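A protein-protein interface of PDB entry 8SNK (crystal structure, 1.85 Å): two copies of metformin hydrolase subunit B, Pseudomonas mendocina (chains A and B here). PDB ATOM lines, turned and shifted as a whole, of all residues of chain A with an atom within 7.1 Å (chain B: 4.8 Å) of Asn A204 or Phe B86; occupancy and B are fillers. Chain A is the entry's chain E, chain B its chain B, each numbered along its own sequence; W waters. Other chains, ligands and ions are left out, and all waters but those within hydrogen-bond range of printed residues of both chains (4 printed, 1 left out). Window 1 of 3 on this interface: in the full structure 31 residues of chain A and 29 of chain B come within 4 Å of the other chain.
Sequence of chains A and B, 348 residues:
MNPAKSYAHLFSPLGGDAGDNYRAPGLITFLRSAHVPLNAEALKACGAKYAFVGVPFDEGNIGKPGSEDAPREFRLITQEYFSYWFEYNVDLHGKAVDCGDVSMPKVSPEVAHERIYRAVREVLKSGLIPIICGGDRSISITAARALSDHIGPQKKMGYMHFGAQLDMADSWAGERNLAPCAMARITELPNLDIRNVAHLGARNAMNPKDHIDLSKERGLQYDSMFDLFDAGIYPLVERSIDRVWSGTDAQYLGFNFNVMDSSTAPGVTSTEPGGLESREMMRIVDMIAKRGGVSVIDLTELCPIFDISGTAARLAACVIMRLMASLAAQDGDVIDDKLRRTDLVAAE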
ATOM      1  N   ALA A 164     -23.810  15.467 -16.448  1.00  0.00           N
ATOM      2  CA  ALA A 164     -23.375  16.599 -15.619  1.00  0.00           C
ATOM      3  C   ALA A 164     -24.217  16.834 -14.358  1.00  0.00           C
ATOM      4  O   ALA A 164     -23.793  17.579 -13.456  1.00  0.00           O
ATOM      5  CB  ALA A 164     -23.329  17.856 -16.436  1.00  0.00           C
ATOM      6  N   LEU A 166     -26.479  15.114 -11.071  1.00  0.00           N
ATOM      7  CA  LEU A 166     -26.751  13.923 -10.263  1.00  0.00           C
ATOM      8  C   LEU A 166     -28.214  13.446 -10.361  1.00  0.00           C
ATOM      9  O   LEU A 166     -28.487  12.241 -10.297  1.00  0.00           O
ATOM     10  CB  LEU A 166     -26.424  14.259  -8.816  1.00  0.00           C
ATOM     11  CG  LEU A 166     -24.951  14.395  -8.484  1.00  0.00           C
ATOM     12  CD1 LEU A 166     -24.787  14.913  -7.079  1.00  0.00           C
ATOM     13  CD2 LEU A 166     -24.217  13.101  -8.651  1.00  0.00           C
ATOM     14  N   GLY A 201     -19.460  12.278 -14.173  1.00  0.00           N
ATOM     15  CA  GLY A 201     -19.353  13.541 -14.898  1.00  0.00           C
ATOM     16  C   GLY A 201     -19.981  14.755 -14.189  1.00  0.00           C
ATOM     17  O   GLY A 201     -19.959  15.863 -14.717  1.00  0.00           O
ATOM     18  N   ALA A 202     -20.492  14.605 -12.961  1.00  0.00           N
ATOM     19  CA  ALA A 202     -21.256  15.694 -12.387  1.00  0.00           C
ATOM     20  C   ALA A 202     -20.359  16.922 -12.212  1.00  0.00           C
ATOM     21  O   ALA A 202     -19.202  16.812 -11.784  1.00  0.00           O
ATOM     22  CB  ALA A 202     -21.852  15.304 -11.075  1.00  0.00           C
ATOM     23  N   ARG A 203     -20.923  18.094 -12.464  1.00  0.00           N
ATOM     24  CA  ARG A 203     -20.136  19.331 -12.399  1.00  0.00           C
ATOM     25  C   ARG A 203     -21.064  20.524 -12.515  1.00  0.00           C
ATOM     26  O   ARG A 203     -22.183  20.355 -12.965  1.00  0.00           O
ATOM     27  CB  ARG A 203     -19.123  19.448 -13.547  1.00  0.00           C
ATOM     28  CG  ARG A 203     -19.745  19.562 -14.937  1.00  0.00           C
ATOM     29  CD  ARG A 203     -18.677  19.387 -16.028  1.00  0.00           C
ATOM     30  NE  ARG A 203     -19.140  19.526 -17.402  1.00  0.00           N
ATOM     31  CZ  ARG A 203     -19.653  18.524 -18.096  1.00  0.00           C
ATOM     32  NH1 ARG A 203     -19.792  17.354 -17.511  1.00  0.00           N
ATOM     33  NH2 ARG A 203     -20.054  18.687 -19.332  1.00  0.00           N
ATOM     34  N   ASN A 204     -20.532  21.727 -12.192  1.00  0.00           N
ATOM     35  CA  ASN A 204     -21.196  23.008 -12.350  1.00  0.00           C
ATOM     36  C   ASN A 204     -22.398  23.089 -11.415  1.00  0.00           C
ATOM     37  O   ASN A 204     -22.433  22.365 -10.426  1.00  0.00           O
ATOM     38  CB  ASN A 204     -21.431  23.356 -13.821  1.00  0.00           C
ATOM     39  CG  ASN A 204     -20.125  23.393 -14.582  1.00  0.00           C
ATOM     40  OD1 ASN A 204     -19.066  23.628 -14.001  1.00  0.00           O
ATOM     41  ND2 ASN A 204     -20.205  23.160 -15.881  1.00  0.00           N
ATOM     42  N   ALA A 205     -23.333  24.014 -11.655  1.00  0.00           N
ATOM     43  CA  ALA A 205     -24.234  24.449 -10.588  1.00  0.00           C
ATOM     44  C   ALA A 205     -25.620  23.790 -10.595  1.00  0.00           C
ATOM     45  O   ALA A 205     -26.318  23.890  -9.566  1.00  0.00           O
ATOM     46  CB  ALA A 205     -24.392  25.950 -10.593  1.00  0.00           C
ATOM     47  N   MET A 206     -25.994  23.041 -11.638  1.00  0.00           N
ATOM     48  CA  MET A 206     -27.333  22.460 -11.702  1.00  0.00           C
ATOM     49  C   MET A 206     -27.407  21.220 -10.799  1.00  0.00           C
ATOM     50  O   MET A 206     -27.948  20.183 -11.189  1.00  0.00           O
ATOM     51  CB  MET A 206     -27.748  22.102 -13.140  1.00  0.00           C
ATOM     52  CG  MET A 206     -27.634  23.253 -14.178  1.00  0.00           C
ATOM     53  SD  MET A 206     -28.223  24.965 -13.699  1.00  0.00           S
ATOM     54  CE  MET A 206     -28.935  25.435 -15.279  1.00  0.00           C
ATOM     55  N   ASN A 207     -26.871  21.347  -9.580  1.00  0.00           N
ATOM     56  CA  ASN A 207     -26.750  20.283  -8.607  1.00  0.00           C
ATOM     57  C   ASN A 207     -27.007  20.830  -7.196  1.00  0.00           C
ATOM     58  O   ASN A 207     -26.080  20.971  -6.389  1.00  0.00           O
ATOM     59  CB  ASN A 207     -25.394  19.585  -8.660  1.00  0.00           C
ATOM     60  CG  ASN A 207     -25.195  18.781  -9.927  1.00  0.00           C
ATOM     61  OD1 ASN A 207     -25.753  17.682 -10.061  1.00  0.00           O
ATOM     62  ND2 ASN A 207     -24.420  19.329 -10.866  1.00  0.00           N
ATOM     63  N   PRO A 208     -28.287  21.050  -6.807  1.00  0.00           N
ATOM     64  CA  PRO A 208     -28.621  21.622  -5.500  1.00  0.00           C
ATOM     65  C   PRO A 208     -28.113  20.797  -4.322  1.00  0.00           C
ATOM     66  O   PRO A 208     -27.890  19.594  -4.443  1.00  0.00           O
ATOM     67  CB  PRO A 208     -30.160  21.679  -5.502  1.00  0.00           C
ATOM     68  CG  PRO A 208     -30.528  21.663  -6.952  1.00  0.00           C
ATOM     69  CD  PRO A 208     -29.494  20.773  -7.598  1.00  0.00           C
ATOM     70  N   LYS A 209     -27.947  21.460  -3.177  1.00  0.00           N
ATOM     71  CA  LYS A 209     -27.254  20.874  -2.052  1.00  0.00           C
ATOM     72  C   LYS A 209     -27.920  19.573  -1.603  1.00  0.00           C
ATOM     73  O   LYS A 209     -27.226  18.676  -1.134  1.00  0.00           O
ATOM     74  CB  LYS A 209     -27.191  21.868  -0.891  1.00  0.00           C
ATOM     75  CG  LYS A 209     -26.435  21.378   0.323  1.00  0.00           C
ATOM     76  CD  LYS A 209     -26.546  22.326   1.495  1.00  0.00           C
ATOM     77  CE  LYS A 209     -25.597  21.971   2.613  1.00  0.00           C
ATOM     78  NZ  LYS A 209     -25.930  20.656   3.210  1.00  0.00           N
ATOM     79  N   ILE A 212     -26.480  16.455  -3.163  1.00  0.00           N
ATOM     80  CA  ILE A 212     -25.274  15.982  -2.506  1.00  0.00           C
ATOM     81  C   ILE A 212     -25.674  15.294  -1.193  1.00  0.00           C
ATOM     82  O   ILE A 212     -25.098  14.257  -0.882  1.00  0.00           O
ATOM     83  CB  ILE A 212     -24.217  17.089  -2.271  1.00  0.00           C
ATOM     84  CG1 ILE A 212     -23.921  17.899  -3.532  1.00  0.00           C
ATOM     85  CG2 ILE A 212     -22.933  16.541  -1.658  1.00  0.00           C
ATOM     86  CD1 ILE A 212     -24.023  17.171  -4.794  1.00  0.00           C
ATOM     87  N   TYR A 222     -20.591   8.726  -6.463  1.00  0.00           N
ATOM     88  CA  TYR A 222     -20.497   9.361  -7.780  1.00  0.00           C
ATOM     89  C   TYR A 222     -19.066   9.824  -8.070  1.00  0.00           C
ATOM     90  O   TYR A 222     -18.272  10.140  -7.174  1.00  0.00           O
ATOM     91  CB  TYR A 222     -21.475  10.528  -7.918  1.00  0.00           C
ATOM     92  CG  TYR A 222     -21.323  11.660  -6.937  1.00  0.00           C
ATOM     93  CD1 TYR A 222     -20.528  12.766  -7.231  1.00  0.00           C
ATOM     94  CD2 TYR A 222     -22.064  11.696  -5.769  1.00  0.00           C
ATOM     95  CE1 TYR A 222     -20.425  13.833  -6.365  1.00  0.00           C
ATOM     96  CE2 TYR A 222     -21.950  12.747  -4.871  1.00  0.00           C
ATOM     97  CZ  TYR A 222     -21.141  13.828  -5.178  1.00  0.00           C
ATOM     98  OH  TYR A 222     -21.000  14.874  -4.297  1.00  0.00           O
ATOM     99  N   SER A 224     -17.390  12.730  -9.697  1.00  0.00           N
ATOM    100  CA  SER A 224     -17.555  14.076 -10.241  1.00  0.00           C
ATOM    101  C   SER A 224     -16.560  14.273 -11.397  1.00  0.00           C
ATOM    102  O   SER A 224     -15.605  13.525 -11.498  1.00  0.00           O
ATOM    103  CB  SER A 224     -17.345  15.116  -9.171  1.00  0.00           C
ATOM    104  OG  SER A 224     -15.953  15.153  -8.823  1.00  0.00           O
ATOM    105  N   MET A 225     -16.838  15.194 -12.328  1.00  0.00           N
ATOM    106  CA  MET A 225     -15.927  15.432 -13.436  1.00  0.00           C
ATOM    107  C   MET A 225     -14.537  15.823 -12.908  1.00  0.00           C
ATOM    108  O   MET A 225     -13.519  15.395 -13.455  1.00  0.00           O
ATOM    109  CB  MET A 225     -16.464  16.556 -14.313  1.00  0.00           C
ATOM    110  CG  MET A 225     -15.799  16.611 -15.644  1.00  0.00           C
ATOM    111  SD  MET A 225     -16.067  15.171 -16.662  1.00  0.00           S
ATOM    112  CE  MET A 225     -17.625  15.457 -17.457  1.00  0.00           C
ATOM    113  N   PHE A 226     -14.492  16.553 -11.791  1.00  0.00           N
ATOM    114  CA  PHE A 226     -13.223  16.967 -11.196  1.00  0.00           C
ATOM    115  C   PHE A 226     -12.480  15.787 -10.572  1.00  0.00           C
ATOM    116  O   PHE A 226     -11.290  15.678 -10.790  1.00  0.00           O
ATOM    117  CB  PHE A 226     -13.397  18.184 -10.282  1.00  0.00           C
ATOM    118  CG  PHE A 226     -13.106  19.504 -10.982  1.00  0.00           C
ATOM    119  CD1 PHE A 226     -12.273  20.458 -10.397  1.00  0.00           C
ATOM    120  CD2 PHE A 226     -13.626  19.789 -12.249  1.00  0.00           C
ATOM    121  CE1 PHE A 226     -11.999  21.661 -11.040  1.00  0.00           C
ATOM    122  CE2 PHE A 226     -13.337  20.986 -12.896  1.00  0.00           C
ATOM    123  CZ  PHE A 226     -12.525  21.920 -12.290  1.00  0.00           C
ATOM    124  N   THR A 271     -26.415  22.001 -21.934  1.00  0.00           N
ATOM    125  CA  THR A 271     -24.981  21.819 -22.156  1.00  0.00           C
ATOM    126  C   THR A 271     -24.220  22.429 -20.998  1.00  0.00           C
ATOM    127  O   THR A 271     -24.702  23.333 -20.376  1.00  0.00           O
ATOM    128  CB  THR A 271     -24.384  22.470 -23.412  1.00  0.00           C
ATOM    129  OG1 THR A 271     -24.608  23.879 -23.385  1.00  0.00           O
ATOM    130  CG2 THR A 271     -24.922  21.916 -24.705  1.00  0.00           C
ATOM    131  N   GLU A 272     -23.022  21.915 -20.745  1.00  0.00           N
ATOM    132  CA  GLU A 272     -22.191  22.347 -19.633  1.00  0.00           C
ATOM    133  C   GLU A 272     -20.748  22.353 -20.099  1.00  0.00           C
ATOM    134  O   GLU A 272     -20.217  21.343 -20.568  1.00  0.00           O
ATOM    135  CB  GLU A 272     -22.353  21.401 -18.441  1.00  0.00           C
ATOM    136  CG  GLU A 272     -23.665  21.507 -17.729  1.00  0.00           C
ATOM    137  CD  GLU A 272     -23.823  22.815 -16.989  1.00  0.00           C
ATOM    138  OE1 GLU A 272     -22.897  23.616 -17.023  1.00  0.00           O
ATOM    139  OE2 GLU A 272     -24.875  23.032 -16.395  1.00  0.00           O
ATOM    140  N   PRO A 273     -20.005  23.468 -19.907  1.00  0.00           N
ATOM    141  CA  PRO A 273     -18.571  23.457 -20.133  1.00  0.00           C
ATOM    142  C   PRO A 273     -17.851  22.558 -19.140  1.00  0.00           C
ATOM    143  O   PRO A 273     -18.379  22.251 -18.056  1.00  0.00           O
ATOM    144  CB  PRO A 273     -18.137  24.937 -19.954  1.00  0.00           C
ATOM    145  CG  PRO A 273     -19.431  25.720 -19.997  1.00  0.00           C
ATOM    146  CD  PRO A 273     -20.516  24.783 -19.500  1.00  0.00           C
ATOM    147  N   GLY A 274     -16.649  22.137 -19.533  1.00  0.00           N
ATOM    148  CA  GLY A 274     -15.712  21.431 -18.653  1.00  0.00           C
ATOM    149  C   GLY A 274     -15.952  19.920 -18.637  1.00  0.00           C
ATOM    150  O   GLY A 274     -15.722  19.272 -17.628  1.00  0.00           O
ATOM    151  N   GLY A 275     -16.497  19.360 -19.747  1.00  0.00           N
ATOM    152  CA  GLY A 275     -16.804  17.926 -19.833  1.00  0.00           C
ATOM    153  C   GLY A 275     -15.781  17.099 -20.619  1.00  0.00           C
ATOM    154  O   GLY A 275     -14.694  17.554 -20.965  1.00  0.00           O
ATOM    155  N   TYR B  84     -25.893  27.858  -6.140  1.00  0.00           N
ATOM    156  CA  TYR B  84     -25.059  27.019  -5.299  1.00  0.00           C
ATOM    157  C   TYR B  84     -24.164  26.133  -6.165  1.00  0.00           C
ATOM    158  O   TYR B  84     -24.678  25.431  -7.031  1.00  0.00           O
ATOM    159  CB  TYR B  84     -25.906  26.098  -4.408  1.00  0.00           C
ATOM    160  CG  TYR B  84     -25.145  25.185  -3.482  1.00  0.00           C
ATOM    161  CD1 TYR B  84     -24.387  25.686  -2.430  1.00  0.00           C
ATOM    162  CD2 TYR B  84     -25.102  23.818  -3.692  1.00  0.00           C
ATOM    163  CE1 TYR B  84     -23.601  24.859  -1.642  1.00  0.00           C
ATOM    164  CE2 TYR B  84     -24.336  22.985  -2.896  1.00  0.00           C
ATOM    165  CZ  TYR B  84     -23.608  23.495  -1.840  1.00  0.00           C
ATOM    166  OH  TYR B  84     -22.857  22.661  -1.033  1.00  0.00           O
ATOM    167  N   TRP B  85     -22.865  26.134  -5.845  1.00  0.00           N
ATOM    168  CA  TRP B  85     -21.841  25.337  -6.522  1.00  0.00           C
ATOM    169  C   TRP B  85     -21.313  24.249  -5.586  1.00  0.00           C
ATOM    170  O   TRP B  85     -20.454  24.503  -4.723  1.00  0.00           O
ATOM    171  CB  TRP B  85     -20.721  26.291  -7.000  1.00  0.00           C
ATOM    172  CG  TRP B  85     -21.153  27.251  -8.063  1.00  0.00           C
ATOM    173  CD1 TRP B  85     -22.010  28.317  -7.989  1.00  0.00           C
ATOM    174  CD2 TRP B  85     -20.838  27.104  -9.458  1.00  0.00           C
ATOM    175  NE1 TRP B  85     -22.243  28.846  -9.237  1.00  0.00           N
ATOM    176  CE2 TRP B  85     -21.526  28.118 -10.152  1.00  0.00           C
ATOM    177  CE3 TRP B  85     -20.027  26.211 -10.163  1.00  0.00           C
ATOM    178  CZ2 TRP B  85     -21.418  28.255 -11.532  1.00  0.00           C
ATOM    179  CZ3 TRP B  85     -19.935  26.351 -11.528  1.00  0.00           C
ATOM    180  CH2 TRP B  85     -20.648  27.337 -12.198  1.00  0.00           C
ATOM    181  N   PHE B  86     -21.760  22.997  -5.800  1.00  0.00           N
ATOM    182  CA  PHE B  86     -21.380  21.875  -4.949  1.00  0.00           C
ATOM    183  C   PHE B  86     -19.868  21.602  -4.939  1.00  0.00           C
ATOM    184  O   PHE B  86     -19.340  21.128  -3.950  1.00  0.00           O
ATOM    185  CB  PHE B  86     -22.177  20.619  -5.311  1.00  0.00           C
ATOM    186  CG  PHE B  86     -21.590  19.791  -6.427  1.00  0.00           C
ATOM    187  CD1 PHE B  86     -21.878  20.073  -7.749  1.00  0.00           C
ATOM    188  CD2 PHE B  86     -20.732  18.739  -6.153  1.00  0.00           C
ATOM    189  CE1 PHE B  86     -21.324  19.314  -8.763  1.00  0.00           C
ATOM    190  CE2 PHE B  86     -20.176  17.979  -7.173  1.00  0.00           C
ATOM    191  CZ  PHE B  86     -20.495  18.266  -8.470  1.00  0.00           C
ATOM    192  N   GLU B  87     -19.128  21.926  -6.016  1.00  0.00           N
ATOM    193  CA  GLU B  87     -17.708  21.645  -6.072  1.00  0.00           C
ATOM    194  C   GLU B  87     -16.964  22.556  -5.088  1.00  0.00           C
ATOM    195  O   GLU B  87     -15.898  22.188  -4.640  1.00  0.00           O
ATOM    196  CB  GLU B  87     -17.182  21.831  -7.497  1.00  0.00           C
ATOM    197  CG  GLU B  87     -17.781  20.868  -8.519  1.00  0.00           C
ATOM    198  CD  GLU B  87     -17.615  21.329  -9.963  1.00  0.00           C
ATOM    199  OE1 GLU B  87     -18.394  22.167 -10.403  1.00  0.00           O
ATOM    200  OE2 GLU B  87     -16.637  20.932 -10.594  1.00  0.00           O
ATOM    201  N   TYR B  88     -17.549  23.718  -4.738  1.00  0.00           N
ATOM    202  CA  TYR B  88     -16.918  24.657  -3.812  1.00  0.00           C
ATOM    203  C   TYR B  88     -17.662  24.767  -2.474  1.00  0.00           C
ATOM    204  O   TYR B  88     -17.153  25.358  -1.532  1.00  0.00           O
ATOM    205  CB  TYR B  88     -16.840  26.044  -4.451  1.00  0.00           C
ATOM    206  CG  TYR B  88     -16.032  26.079  -5.721  1.00  0.00           C
ATOM    207  CD1 TYR B  88     -14.660  26.151  -5.672  1.00  0.00           C
ATOM    208  CD2 TYR B  88     -16.610  26.029  -6.976  1.00  0.00           C
ATOM    209  CE1 TYR B  88     -13.868  26.173  -6.807  1.00  0.00           C
ATOM    210  CE2 TYR B  88     -15.828  26.066  -8.131  1.00  0.00           C
ATOM    211  CZ  TYR B  88     -14.454  26.134  -8.052  1.00  0.00           C
ATOM    212  OH  TYR B  88     -13.602  26.144  -9.157  1.00  0.00           O
ATOM    213  N   ASN B  89     -18.886  24.276  -2.419  1.00  0.00           N
ATOM    214  CA  ASN B  89     -19.747  24.451  -1.262  1.00  0.00           C
ATOM    215  C   ASN B  89     -19.947  25.932  -0.968  1.00  0.00           C
ATOM    216  O   ASN B  89     -19.952  26.355   0.185  1.00  0.00           O
ATOM    217  CB  ASN B  89     -19.262  23.669  -0.031  1.00  0.00           C
ATOM    218  CG  ASN B  89     -20.310  23.693   1.072  1.00  0.00           C
ATOM    219  OD1 ASN B  89     -21.503  23.540   0.798  1.00  0.00           O
ATOM    220  ND2 ASN B  89     -19.889  23.944   2.307  1.00  0.00           N
ATOM    221  N   MET B 282     -10.615  26.406 -16.359  1.00  0.00           N
ATOM    222  CA  MET B 282     -11.234  26.262 -15.054  1.00  0.00           C
ATOM    223  C   MET B 282     -10.145  25.970 -13.991  1.00  0.00           C
ATOM    224  O   MET B 282     -10.256  26.469 -12.856  1.00  0.00           O
ATOM    225  CB  MET B 282     -12.328  25.199 -15.129  1.00  0.00           C
ATOM    226  CG  MET B 282     -13.553  25.718 -15.929  1.00  0.00           C
ATOM    227  SD  MET B 282     -14.457  24.196 -16.284  1.00  0.00           S
ATOM    228  CE  MET B 282     -15.903  24.861 -17.113  1.00  0.00           C
ATOM    229  N   CYS B 318     -19.582  30.596 -17.110  1.00  0.00           N
ATOM    230  CA  CYS B 318     -19.038  29.600 -16.198  1.00  0.00           C
ATOM    231  C   CYS B 318     -17.674  29.989 -15.638  1.00  0.00           C
ATOM    232  O   CYS B 318     -17.441  29.789 -14.448  1.00  0.00           O
ATOM    233  CB  CYS B 318     -18.965  28.241 -16.854  1.00  0.00           C
ATOM    234  SG  CYS B 318     -20.607  27.483 -16.893  1.00  0.00           S
ATOM    235  N   ARG B 322     -17.414  30.623 -11.679  1.00  0.00           N
ATOM    236  CA  ARG B 322     -16.488  29.726 -11.012  1.00  0.00           C
ATOM    237  C   ARG B 322     -15.398  30.548 -10.323  1.00  0.00           C
ATOM    238  O   ARG B 322     -14.980  30.184  -9.238  1.00  0.00           O
ATOM    239  CB  ARG B 322     -15.889  28.676 -11.969  1.00  0.00           C
ATOM    240  CG  ARG B 322     -16.864  27.557 -12.289  1.00  0.00           C
ATOM    241  CD  ARG B 322     -16.354  26.456 -13.214  1.00  0.00           C
ATOM    242  NE  ARG B 322     -15.389  25.613 -12.534  1.00  0.00           N
ATOM    243  CZ  ARG B 322     -15.690  24.464 -11.964  1.00  0.00           C
ATOM    244  NH1 ARG B 322     -16.840  23.869 -12.222  1.00  0.00           N
ATOM    245  NH2 ARG B 322     -14.828  23.900 -11.160  1.00  0.00           N
HETATM  246  O   HOH W   1     -15.338  20.655 -15.304  1.00  0.00           O
HETATM  247  O   HOH W   2     -20.167  23.135  -8.594  1.00  0.00           O
HETATM  248  O   HOH W   3     -27.296  24.268  -6.980  1.00  0.00           O
HETATM  249  O   HOH W   4     -16.882  18.166 -10.868  1.00  0.00           O
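Water W2 lies within hydrogen-bond range of OE1 of Glu B87 (2.7 Å), O of Asn A204 (3.0 Å) and N of Phe B86 (3.2 Å). Water W1 lies within hydrogen-bond range of the backbone carbonyl oxygen of Gly A274 (2.7 Å) and the side-chain sulfur of Met B282 (3.8 Å). Water W4 lies within hydrogen-bond range of the side-chain carboxylate of Glu B87, the backbone carbonyl oxygen of Ala A202, the backbone NH of Phe A226 and the backbone NH of Met A225. Water W3 lies within hydrogen-bond range of the backbone carbonyl oxygen of Ala A205 (2.8 Å) and the backbone carbonyl oxygen of Tyr B84 (2.9 Å).
N of Asn A204 is in hydrogen-bond range of OE1 of Glu B87 (2.8 Å). NH1 of Arg B322 is in hydrogen-bond range of OD1 of Asn A204, at 2.9 Å. The backbone carbonyl oxygen (O) of Ala A205 sits close to the backbone carbonyl oxygen (O) of Tyr B84, at 3.4 Å.
Of the 21 printed residues of chain A, 10 touch a printed residue of chain B. Hydrophobic or aromatic side chains of chain A that line the printed part of chain B: Ala A205, Ile A212, Phe A226 and Pro A273. Of the 9 printed residues of chain B, 7 touch a printed residue of chain A. Printed residues of chain B that touch a printed residue of chain A: Tyr B84, Trp B85, Phe B86, Glu B87, Met B282, Cys B318 and Arg B322. Among the printed residues, no Asp or Glu carboxylate lies within 4 Å of a Lys or Arg side-chain nitrogen of the other chain.
Of chain B, only Trp B85 (3.7 Å), Phe B86 (3.6 Å), Glu B87 (2.8 Å) and Arg B322 (2.9 Å) come within 4 Å of Asn A204. Phe B86 touches five residues of chain A. Printed residues of chain A within 4 Å of Met B282: Pro A273 (3.6 Å) and Gly A274 (3.7 Å). Of the printed residues of chain A, Glu B87 touches Arg A203, Asn A204 and Phe A226. Of the printed residues of chain B, Lys A209 touches Tyr B84 (3.7 Å). Of the printed residues of chain B, Ala A202 touches Phe B86. Of the printed residues of chain B, Asn A207 touches Phe B86. The nearest residue of chain B that does not touch Asn A204 is Cys B318 (4.5 Å).
Arg A203 touches Phe B86. Asn A204 touches Phe B86. Asn A207 touches Phe B86. CB of Lys A209 touches CE2 of Tyr B84, 3.7 Å away. Phe B86 touches Ile A212. Phe A226 touches Glu B87 (CD2 to OE2, 3.6 Å). Phe A226 touches Arg B322 (CZ to NH2, 3.2 Å). Pro A273 touches Met B282. CD of Pro A273 touches SG of Cys B318, 3.8 Å away. N of Gly A274 touches CE of Met B282, at 3.7 Å.
NH2 of Arg B322 is in hydrogen-bond range of OH of Tyr B88 (3.2 Å). O of Ala A164 is in hydrogen-bond range of N of Arg A203, 3.1 Å away. The guanidinium group (NH2) of Arg A203 is in hydrogen-bond range of the backbone carbonyl oxygen (O) of Glu A272, 2.9 Å away. The backbone carbonyl oxygen (O) of Pro A273 lies within hydrogen-bond range of the guanidinium group (NE) of Arg A203, 2.9 Å away. The side-chain amide nitrogen (ND2) of Asn A204 sits at hydrogen-bond distance from the side-chain carboxylate (OE1) of Glu A272 (3.0 Å). The side-chain amide nitrogen (ND2) of Asn A204 is in hydrogen-bond range of the backbone carbonyl oxygen (O) of Pro A273.
No position is printed for both chains. Of the 17 pairs that touch across the chains among the printed residues, none has its exchanged pair printed and touching as well.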
